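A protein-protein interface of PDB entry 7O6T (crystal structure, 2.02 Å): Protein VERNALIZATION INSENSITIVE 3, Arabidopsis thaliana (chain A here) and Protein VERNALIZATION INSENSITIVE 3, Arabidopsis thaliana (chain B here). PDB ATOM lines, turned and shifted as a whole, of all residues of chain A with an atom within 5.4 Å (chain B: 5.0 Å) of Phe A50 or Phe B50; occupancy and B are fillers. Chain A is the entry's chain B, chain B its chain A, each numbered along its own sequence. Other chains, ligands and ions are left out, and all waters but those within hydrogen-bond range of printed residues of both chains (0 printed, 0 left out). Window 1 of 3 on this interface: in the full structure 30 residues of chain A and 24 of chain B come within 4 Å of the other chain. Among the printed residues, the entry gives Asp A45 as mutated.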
ATOM      1  N   THR A   9      -0.092 -18.056  16.125  1.00  0.00           N
ATOM      2  CA  THR A   9      -1.166 -18.175  17.065  1.00  0.00           C
ATOM      3  C   THR A   9      -1.278 -16.897  17.894  1.00  0.00           C
ATOM      4  O   THR A   9      -2.359 -16.337  18.049  1.00  0.00           O
ATOM      5  CB  THR A   9      -0.928 -19.401  17.978  1.00  0.00           C
ATOM      6  OG1 THR A   9      -1.009 -20.602  17.194  1.00  0.00           O
ATOM      7  CG2 THR A   9      -1.930 -19.451  19.057  1.00  0.00           C
ATOM      8  N   ASP A  45       1.995 -28.217  23.332  1.00  0.00           N
ATOM      9  CA  ASP A  45       0.827 -29.103  23.371  1.00  0.00           C
ATOM     10  C   ASP A  45      -0.497 -28.345  23.183  1.00  0.00           C
ATOM     11  O   ASP A  45      -1.352 -28.780  22.414  1.00  0.00           O
ATOM     12  CB  ASP A  45       0.794 -29.929  24.663  1.00  0.00           C
ATOM     13  CG  ASP A  45       1.952 -30.908  24.764  1.00  0.00           C
ATOM     14  OD1 ASP A  45       2.676 -31.113  23.750  1.00  0.00           O
ATOM     15  OD2 ASP A  45       2.146 -31.476  25.878  1.00  0.00           O
ATOM     16  N   PHE A  46      -0.660 -27.207  23.870  1.00  0.00           N
ATOM     17  CA  PHE A  46      -1.856 -26.380  23.695  1.00  0.00           C
ATOM     18  C   PHE A  46      -2.027 -25.934  22.223  1.00  0.00           C
ATOM     19  O   PHE A  46      -3.104 -26.042  21.639  1.00  0.00           O
ATOM     20  CB  PHE A  46      -1.835 -25.151  24.596  1.00  0.00           C
ATOM     21  CG  PHE A  46      -2.199 -25.417  26.027  1.00  0.00           C
ATOM     22  CD1 PHE A  46      -3.316 -26.188  26.355  1.00  0.00           C
ATOM     23  CD2 PHE A  46      -1.479 -24.816  27.067  1.00  0.00           C
ATOM     24  CE1 PHE A  46      -3.673 -26.378  27.684  1.00  0.00           C
ATOM     25  CE2 PHE A  46      -1.824 -25.017  28.380  1.00  0.00           C
ATOM     26  CZ  PHE A  46      -2.930 -25.800  28.699  1.00  0.00           C
ATOM     27  N   VAL A  47      -0.933 -25.457  21.631  1.00  0.00           N
ATOM     28  CA  VAL A  47      -0.936 -24.920  20.293  1.00  0.00           C
ATOM     29  C   VAL A  47      -1.140 -26.035  19.271  1.00  0.00           C
ATOM     30  O   VAL A  47      -1.916 -25.892  18.353  1.00  0.00           O
ATOM     31  CB  VAL A  47       0.352 -24.109  20.022  1.00  0.00           C
ATOM     32  CG1 VAL A  47       0.449 -23.731  18.542  1.00  0.00           C
ATOM     33  CG2 VAL A  47       0.355 -22.862  20.877  1.00  0.00           C
ATOM     34  N   GLU A  48      -0.440 -27.154  19.471  1.00  0.00           N
ATOM     35  CA  GLU A  48      -0.582 -28.362  18.683  1.00  0.00           C
ATOM     36  C   GLU A  48      -2.037 -28.837  18.617  1.00  0.00           C
ATOM     37  O   GLU A  48      -2.539 -29.140  17.543  1.00  0.00           O
ATOM     38  CB  GLU A  48       0.314 -29.459  19.269  1.00  0.00           C
ATOM     39  CG  GLU A  48       0.257 -30.804  18.553  1.00  0.00           C
ATOM     40  CD  GLU A  48       0.688 -31.969  19.441  1.00  0.00           C
ATOM     41  OE1 GLU A  48       0.691 -31.842  20.690  1.00  0.00           O
ATOM     42  OE2 GLU A  48       0.988 -33.041  18.873  1.00  0.00           O
ATOM     43  N   THR A  49      -2.713 -28.881  19.768  1.00  0.00           N
ATOM     44  CA  THR A  49      -4.119 -29.265  19.852  1.00  0.00           C
ATOM     45  C   THR A  49      -4.958 -28.341  19.004  1.00  0.00           C
ATOM     46  O   THR A  49      -5.824 -28.797  18.223  1.00  0.00           O
ATOM     47  CB  THR A  49      -4.633 -29.252  21.309  1.00  0.00           C
ATOM     48  OG1 THR A  49      -3.946 -30.270  22.033  1.00  0.00           O
ATOM     49  CG2 THR A  49      -6.114 -29.527  21.387  1.00  0.00           C
ATOM     50  N   PHE A  50      -4.698 -27.040  19.140  1.00  0.00           N
ATOM     51  CA  PHE A  50      -5.404 -26.044  18.364  1.00  0.00           C
ATOM     52  C   PHE A  50      -5.187 -26.225  16.849  1.00  0.00           C
ATOM     53  O   PHE A  50      -6.140 -26.143  16.079  1.00  0.00           O
ATOM     54  CB  PHE A  50      -4.990 -24.651  18.790  1.00  0.00           C
ATOM     55  CG  PHE A  50      -5.624 -23.577  17.987  1.00  0.00           C
ATOM     56  CD1 PHE A  50      -6.924 -23.215  18.251  1.00  0.00           C
ATOM     57  CD2 PHE A  50      -4.931 -22.924  16.976  1.00  0.00           C
ATOM     58  CE1 PHE A  50      -7.545 -22.208  17.539  1.00  0.00           C
ATOM     59  CE2 PHE A  50      -5.555 -21.934  16.232  1.00  0.00           C
ATOM     60  CZ  PHE A  50      -6.863 -21.580  16.523  1.00  0.00           C
ATOM     61  N   MET A  51      -3.941 -26.459  16.431  1.00  0.00           N
ATOM     62  CA  MET A  51      -3.580 -26.655  14.997  1.00  0.00           C
ATOM     63  C   MET A  51      -4.236 -27.948  14.485  1.00  0.00           C
ATOM     64  O   MET A  51      -4.669 -27.952  13.347  1.00  0.00           O
ATOM     65  CB  MET A  51      -2.060 -26.692  14.773  1.00  0.00           C
ATOM     66  CG  MET A  51      -1.284 -25.408  15.136  1.00  0.00           C
ATOM     67  SD  MET A  51      -2.049 -23.881  14.135  1.00  0.00           S
ATOM     68  CE  MET A  51      -0.921 -22.323  14.521  1.00  0.00           C
ATOM     69  N   GLU A  52      -4.322 -29.003  15.301  1.00  0.00           N
ATOM     70  CA  GLU A  52      -5.018 -30.232  14.926  1.00  0.00           C
ATOM     71  C   GLU A  52      -6.530 -30.003  14.739  1.00  0.00           C
ATOM     72  O   GLU A  52      -7.119 -30.506  13.775  1.00  0.00           O
ATOM     73  CB  GLU A  52      -4.799 -31.337  15.960  1.00  0.00           C
ATOM     74  CG  GLU A  52      -3.401 -31.921  15.964  1.00  0.00           C
ATOM     75  CD  GLU A  52      -3.128 -32.806  17.176  1.00  0.00           C
ATOM     76  OE1 GLU A  52      -4.012 -32.925  18.068  1.00  0.00           O
ATOM     77  OE2 GLU A  52      -2.020 -33.394  17.228  1.00  0.00           O
ATOM     78  N   ASP A  53      -7.146 -29.241  15.653  1.00  0.00           N
ATOM     79  CA  ASP A  53      -8.562 -28.894  15.555  1.00  0.00           C
ATOM     80  C   ASP A  53      -8.854 -28.034  14.312  1.00  0.00           C
ATOM     81  O   ASP A  53      -9.863 -28.222  13.661  1.00  0.00           O
ATOM     82  CB  ASP A  53      -9.071 -28.199  16.811  1.00  0.00           C
ATOM     83  CG  ASP A  53      -9.048 -29.114  18.055  1.00  0.00           C
ATOM     84  OD1 ASP A  53      -8.774 -30.334  17.952  1.00  0.00           O
ATOM     85  OD2 ASP A  53      -9.279 -28.591  19.156  1.00  0.00           O
ATOM     86  N   LEU A  54      -7.961 -27.094  14.008  1.00  0.00           N
ATOM     87  CA  LEU A  54      -8.009 -26.320  12.777  1.00  0.00           C
ATOM     88  C   LEU A  54      -7.916 -27.203  11.511  1.00  0.00           C
ATOM     89  O   LEU A  54      -8.651 -27.006  10.549  1.00  0.00           O
ATOM     90  CB  LEU A  54      -6.906 -25.259  12.773  1.00  0.00           C
ATOM     91  CG  LEU A  54      -6.895 -24.297  11.592  1.00  0.00           C
ATOM     92  CD1 LEU A  54      -8.219 -23.553  11.473  1.00  0.00           C
ATOM     93  CD2 LEU A  54      -5.751 -23.311  11.683  1.00  0.00           C
ATOM     94  N   SER A  55      -6.979 -28.155  11.502  1.00  0.00           N
ATOM     95  CA  SER A  55      -6.877 -29.124  10.414  1.00  0.00           C
ATOM     96  C   SER A  55      -8.188 -29.902  10.233  1.00  0.00           C
ATOM     97  O   SER A  55      -8.674 -30.036   9.132  1.00  0.00           O
ATOM     98  CB  SER A  55      -5.721 -30.094  10.652  1.00  0.00           C
ATOM     99  OG  SER A  55      -5.613 -31.006   9.582  1.00  0.00           O
ATOM    100  N   LEU A  57     -11.230 -29.061  11.218  1.00  0.00           N
ATOM    101  CA  LEU A  57     -12.208 -28.098  10.708  1.00  0.00           C
ATOM    102  C   LEU A  57     -12.104 -27.976   9.170  1.00  0.00           C
ATOM    103  O   LEU A  57     -13.096 -28.057   8.458  1.00  0.00           O
ATOM    104  CB  LEU A  57     -12.001 -26.724  11.381  1.00  0.00           C
ATOM    105  CG  LEU A  57     -12.687 -25.489  10.763  1.00  0.00           C
ATOM    106  CD1 LEU A  57     -14.185 -25.666  10.818  1.00  0.00           C
ATOM    107  CD2 LEU A  57     -12.301 -24.198  11.474  1.00  0.00           C
ATOM    108  N   THR B   9     -11.856 -17.527   9.385  1.00  0.00           N
ATOM    109  CA  THR B   9     -11.629 -18.951   9.482  1.00  0.00           C
ATOM    110  C   THR B   9     -11.015 -19.458   8.176  1.00  0.00           C
ATOM    111  O   THR B   9     -10.035 -20.210   8.164  1.00  0.00           O
ATOM    112  CB  THR B   9     -12.954 -19.675   9.775  1.00  0.00           C
ATOM    113  OG1 THR B   9     -13.441 -19.313  11.078  1.00  0.00           O
ATOM    114  CG2 THR B   9     -12.753 -21.160   9.753  1.00  0.00           C
ATOM    115  N   CME B  12      -7.452 -18.327   7.800  1.00  0.00           N
ATOM    116  CA  CME B  12      -6.658 -19.187   8.711  1.00  0.00           C
ATOM    117  CB  CME B  12      -7.357 -19.394  10.042  1.00  0.00           C
ATOM    118  SG  CME B  12      -7.036 -18.104  11.265  1.00  0.00           S
ATOM    119  SD  CME B  12      -5.014 -18.159  11.373  1.00  0.00           S
ATOM    120  CE  CME B  12      -4.728 -19.009  12.955  1.00  0.00           C
ATOM    121  CZ  CME B  12      -3.429 -19.752  12.973  1.00  0.00           C
ATOM    122  OH  CME B  12      -2.790 -19.639  11.717  1.00  0.00           O
ATOM    123  C   CME B  12      -6.345 -20.526   8.037  1.00  0.00           C
ATOM    124  O   CME B  12      -5.162 -20.928   8.018  1.00  0.00           O
ATOM    125  N   PHE B  46     -19.370 -24.901  12.820  1.00  0.00           N
ATOM    126  CA  PHE B  46     -17.925 -25.155  12.766  1.00  0.00           C
ATOM    127  C   PHE B  46     -17.103 -23.910  13.102  1.00  0.00           C
ATOM    128  O   PHE B  46     -16.151 -23.974  13.875  1.00  0.00           O
ATOM    129  CB  PHE B  46     -17.462 -25.728  11.416  1.00  0.00           C
ATOM    130  CG  PHE B  46     -17.918 -27.139  11.133  1.00  0.00           C
ATOM    131  CD1 PHE B  46     -18.081 -28.096  12.147  1.00  0.00           C
ATOM    132  CD2 PHE B  46     -18.159 -27.520   9.834  1.00  0.00           C
ATOM    133  CE1 PHE B  46     -18.507 -29.377  11.850  1.00  0.00           C
ATOM    134  CE2 PHE B  46     -18.570 -28.809   9.526  1.00  0.00           C
ATOM    135  CZ  PHE B  46     -18.747 -29.737  10.531  1.00  0.00           C
ATOM    136  N   VAL B  47     -17.490 -22.777  12.524  1.00  0.00           N
ATOM    137  CA  VAL B  47     -16.776 -21.512  12.692  1.00  0.00           C
ATOM    138  C   VAL B  47     -16.898 -20.992  14.131  1.00  0.00           C
ATOM    139  O   VAL B  47     -15.913 -20.534  14.714  1.00  0.00           O
ATOM    140  CB  VAL B  47     -17.335 -20.492  11.674  1.00  0.00           C
ATOM    141  CG1 VAL B  47     -16.946 -19.064  12.002  1.00  0.00           C
ATOM    142  CG2 VAL B  47     -16.864 -20.898  10.280  1.00  0.00           C
ATOM    143  N   GLU B  48     -18.105 -21.085  14.695  1.00  0.00           N
ATOM    144  CA  GLU B  48     -18.372 -20.700  16.085  1.00  0.00           C
ATOM    145  C   GLU B  48     -17.470 -21.461  17.053  1.00  0.00           C
ATOM    146  O   GLU B  48     -16.829 -20.861  17.938  1.00  0.00           O
ATOM    147  CB  GLU B  48     -19.830 -20.936  16.424  1.00  0.00           C
ATOM    148  CG  GLU B  48     -20.213 -20.441  17.803  1.00  0.00           C
ATOM    149  CD  GLU B  48     -21.698 -20.638  18.112  1.00  0.00           C
ATOM    150  OE1 GLU B  48     -22.480 -20.952  17.181  1.00  0.00           O
ATOM    151  OE2 GLU B  48     -22.090 -20.463  19.284  1.00  0.00           O
ATOM    152  N   THR B  49     -17.388 -22.776  16.848  1.00  0.00           N
ATOM    153  CA  THR B  49     -16.506 -23.637  17.616  1.00  0.00           C
ATOM    154  C   THR B  49     -15.066 -23.169  17.534  1.00  0.00           C
ATOM    155  O   THR B  49     -14.379 -23.078  18.547  1.00  0.00           O
ATOM    156  CB  THR B  49     -16.615 -25.104  17.157  1.00  0.00           C
ATOM    157  OG1 THR B  49     -17.942 -25.575  17.394  1.00  0.00           O
ATOM    158  CG2 THR B  49     -15.622 -25.999  17.907  1.00  0.00           C
ATOM    159  N   PHE B  50     -14.611 -22.855  16.321  1.00  0.00           N
ATOM    160  CA  PHE B  50     -13.262 -22.358  16.104  1.00  0.00           C
ATOM    161  C   PHE B  50     -12.999 -21.044  16.848  1.00  0.00           C
ATOM    162  O   PHE B  50     -11.936 -20.887  17.456  1.00  0.00           O
ATOM    163  CB  PHE B  50     -12.986 -22.195  14.624  1.00  0.00           C
ATOM    164  CG  PHE B  50     -11.683 -21.525  14.308  1.00  0.00           C
ATOM    165  CD1 PHE B  50     -10.484 -22.196  14.442  1.00  0.00           C
ATOM    166  CD2 PHE B  50     -11.669 -20.230  13.885  1.00  0.00           C
ATOM    167  CE1 PHE B  50      -9.286 -21.571  14.171  1.00  0.00           C
ATOM    168  CE2 PHE B  50     -10.469 -19.595  13.563  1.00  0.00           C
ATOM    169  CZ  PHE B  50      -9.278 -20.281  13.687  1.00  0.00           C
ATOM    170  N   MET B  51     -13.948 -20.103  16.805  1.00  0.00           N
ATOM    171  CA  MET B  51     -13.786 -18.781  17.482  1.00  0.00           C
ATOM    172  C   MET B  51     -13.738 -19.013  19.012  1.00  0.00           C
ATOM    173  O   MET B  51     -12.900 -18.364  19.701  1.00  0.00           O
ATOM    174  CB  MET B  51     -14.898 -17.807  17.067  1.00  0.00           C
ATOM    175  CG  MET B  51     -14.995 -17.480  15.574  1.00  0.00           C
ATOM    176  SD  MET B  51     -13.305 -16.621  15.024  1.00  0.00           S
ATOM    177  CE  MET B  51     -12.776 -16.990  13.181  1.00  0.00           C
ATOM    178  N   GLU B  52     -14.556 -19.940  19.525  1.00  0.00           N
ATOM    179  CA  GLU B  52     -14.535 -20.306  20.953  1.00  0.00           C
ATOM    180  C   GLU B  52     -13.184 -20.948  21.373  1.00  0.00           C
ATOM    181  O   GLU B  52     -12.632 -20.624  22.428  1.00  0.00           O
ATOM    182  CB  GLU B  52     -15.686 -21.248  21.278  1.00  0.00           C
ATOM    183  CG  GLU B  52     -17.067 -20.606  21.231  1.00  0.00           C
ATOM    184  CD  GLU B  52     -18.210 -21.625  21.264  1.00  0.00           C
ATOM    185  OE1 GLU B  52     -17.929 -22.849  21.322  1.00  0.00           O
ATOM    186  OE2 GLU B  52     -19.395 -21.208  21.213  1.00  0.00           O
ATOM    187  N   ASP B  53     -12.672 -21.864  20.540  1.00  0.00           N
ATOM    188  CA  ASP B  53     -11.364 -22.502  20.747  1.00  0.00           C
ATOM    189  C   ASP B  53     -10.232 -21.537  20.764  1.00  0.00           C
ATOM    190  O   ASP B  53      -9.324 -21.689  21.570  1.00  0.00           O
ATOM    191  CB  ASP B  53     -11.038 -23.536  19.668  1.00  0.00           C
ATOM    192  CG  ASP B  53     -11.883 -24.743  19.755  1.00  0.00           C
ATOM    193  OD1 ASP B  53     -12.627 -24.826  20.732  1.00  0.00           O
ATOM    194  OD2 ASP B  53     -11.802 -25.590  18.830  1.00  0.00           O
ATOM    195  N   LEU B  54     -10.257 -20.564  19.842  1.00  0.00           N
ATOM    196  CA  LEU B  54      -9.280 -19.486  19.817  1.00  0.00           C
ATOM    197  C   LEU B  54      -9.283 -18.664  21.147  1.00  0.00           C
ATOM    198  O   LEU B  54      -8.219 -18.356  21.721  1.00  0.00           O
ATOM    199  CB  LEU B  54      -9.544 -18.587  18.617  1.00  0.00           C
ATOM    200  CG  LEU B  54      -8.562 -17.450  18.404  1.00  0.00           C
ATOM    201  CD1 LEU B  54      -7.155 -17.970  18.196  1.00  0.00           C
ATOM    202  CD2 LEU B  54      -9.025 -16.602  17.219  1.00  0.00           C
ATOM    203  N   LEU B  57      -7.807 -20.866  23.925  1.00  0.00           N
ATOM    204  CA  LEU B  57      -6.363 -20.928  23.739  1.00  0.00           C
ATOM    205  C   LEU B  57      -5.684 -19.699  24.351  1.00  0.00           C
ATOM    206  O   LEU B  57      -4.731 -19.828  25.117  1.00  0.00           O
ATOM    207  CB  LEU B  57      -6.010 -21.064  22.248  1.00  0.00           C
ATOM    208  CG  LEU B  57      -4.506 -21.141  21.922  1.00  0.00           C
ATOM    209  CD1 LEU B  57      -3.832 -22.289  22.669  1.00  0.00           C
ATOM    210  CD2 LEU B  57      -4.313 -21.254  20.410  1.00  0.00           C
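Thr A9 touches Leu B57.
Phe A46 touches Leu B57 (O to CD1, 3.96 Å).
Phe A50 touches Phe B50.
Leu B54 touches Phe A50 (N to CE1, 3.9 Å).
Leu B57 touches Phe A50.
CME B12 touches Met A51.
Asp A53 touches Asp B53 (OD2 to OD2, 3.9 Å).
Phe B50 touches Leu A54 (CE1 to CD1, 3.5 Å).
CG2 of Thr B9 touches CD2 of Leu A57, at 3.5 Å.
CD1 of Leu A57 touches CB of Phe B46, 3.3 Å away.
Of the 13 printed residues of chain A, 7 touch a printed residue of chain B.
Along chain A the printed residues that touch a printed residue of chain B span positions 9 to 57.
Printed residues of chain B that touch a printed residue of chain A: Thr B9, CME B12, Phe B46, Phe B50, Asp B53, Leu B54 and Leu B57.
Hydrophobic or aromatic side chains of chain B within 4 Å of the printed part of chain A: Phe B46, Phe B50, Leu B54 and Leu B57.
Among the printed residues, 11 pairs touch across the chains.
Among the printed residues, no Asp or Glu carboxylate lies within 4 Å of a Lys or Arg side-chain nitrogen of the other chain.
Phe A50 touches three residues of chain B.
Phe B50 touches three residues of chain A.
Of the printed residues of chain B, Thr A9 touches Leu B57.
Of the printed residues of chain B, Asp A53 touches Asp B53.
Glu A48 touches none of the printed residues of chain B.
The nearest residue of chain B that does not touch Phe A50 is Asp B53 (4.3 Å).
The nearest printed residue of chain A that does not touch Phe B50 is Asp A53 (6.1 Å).
The nearest printed residue of chain A that does not touch CME B12 is Leu A54 (4.4 Å).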
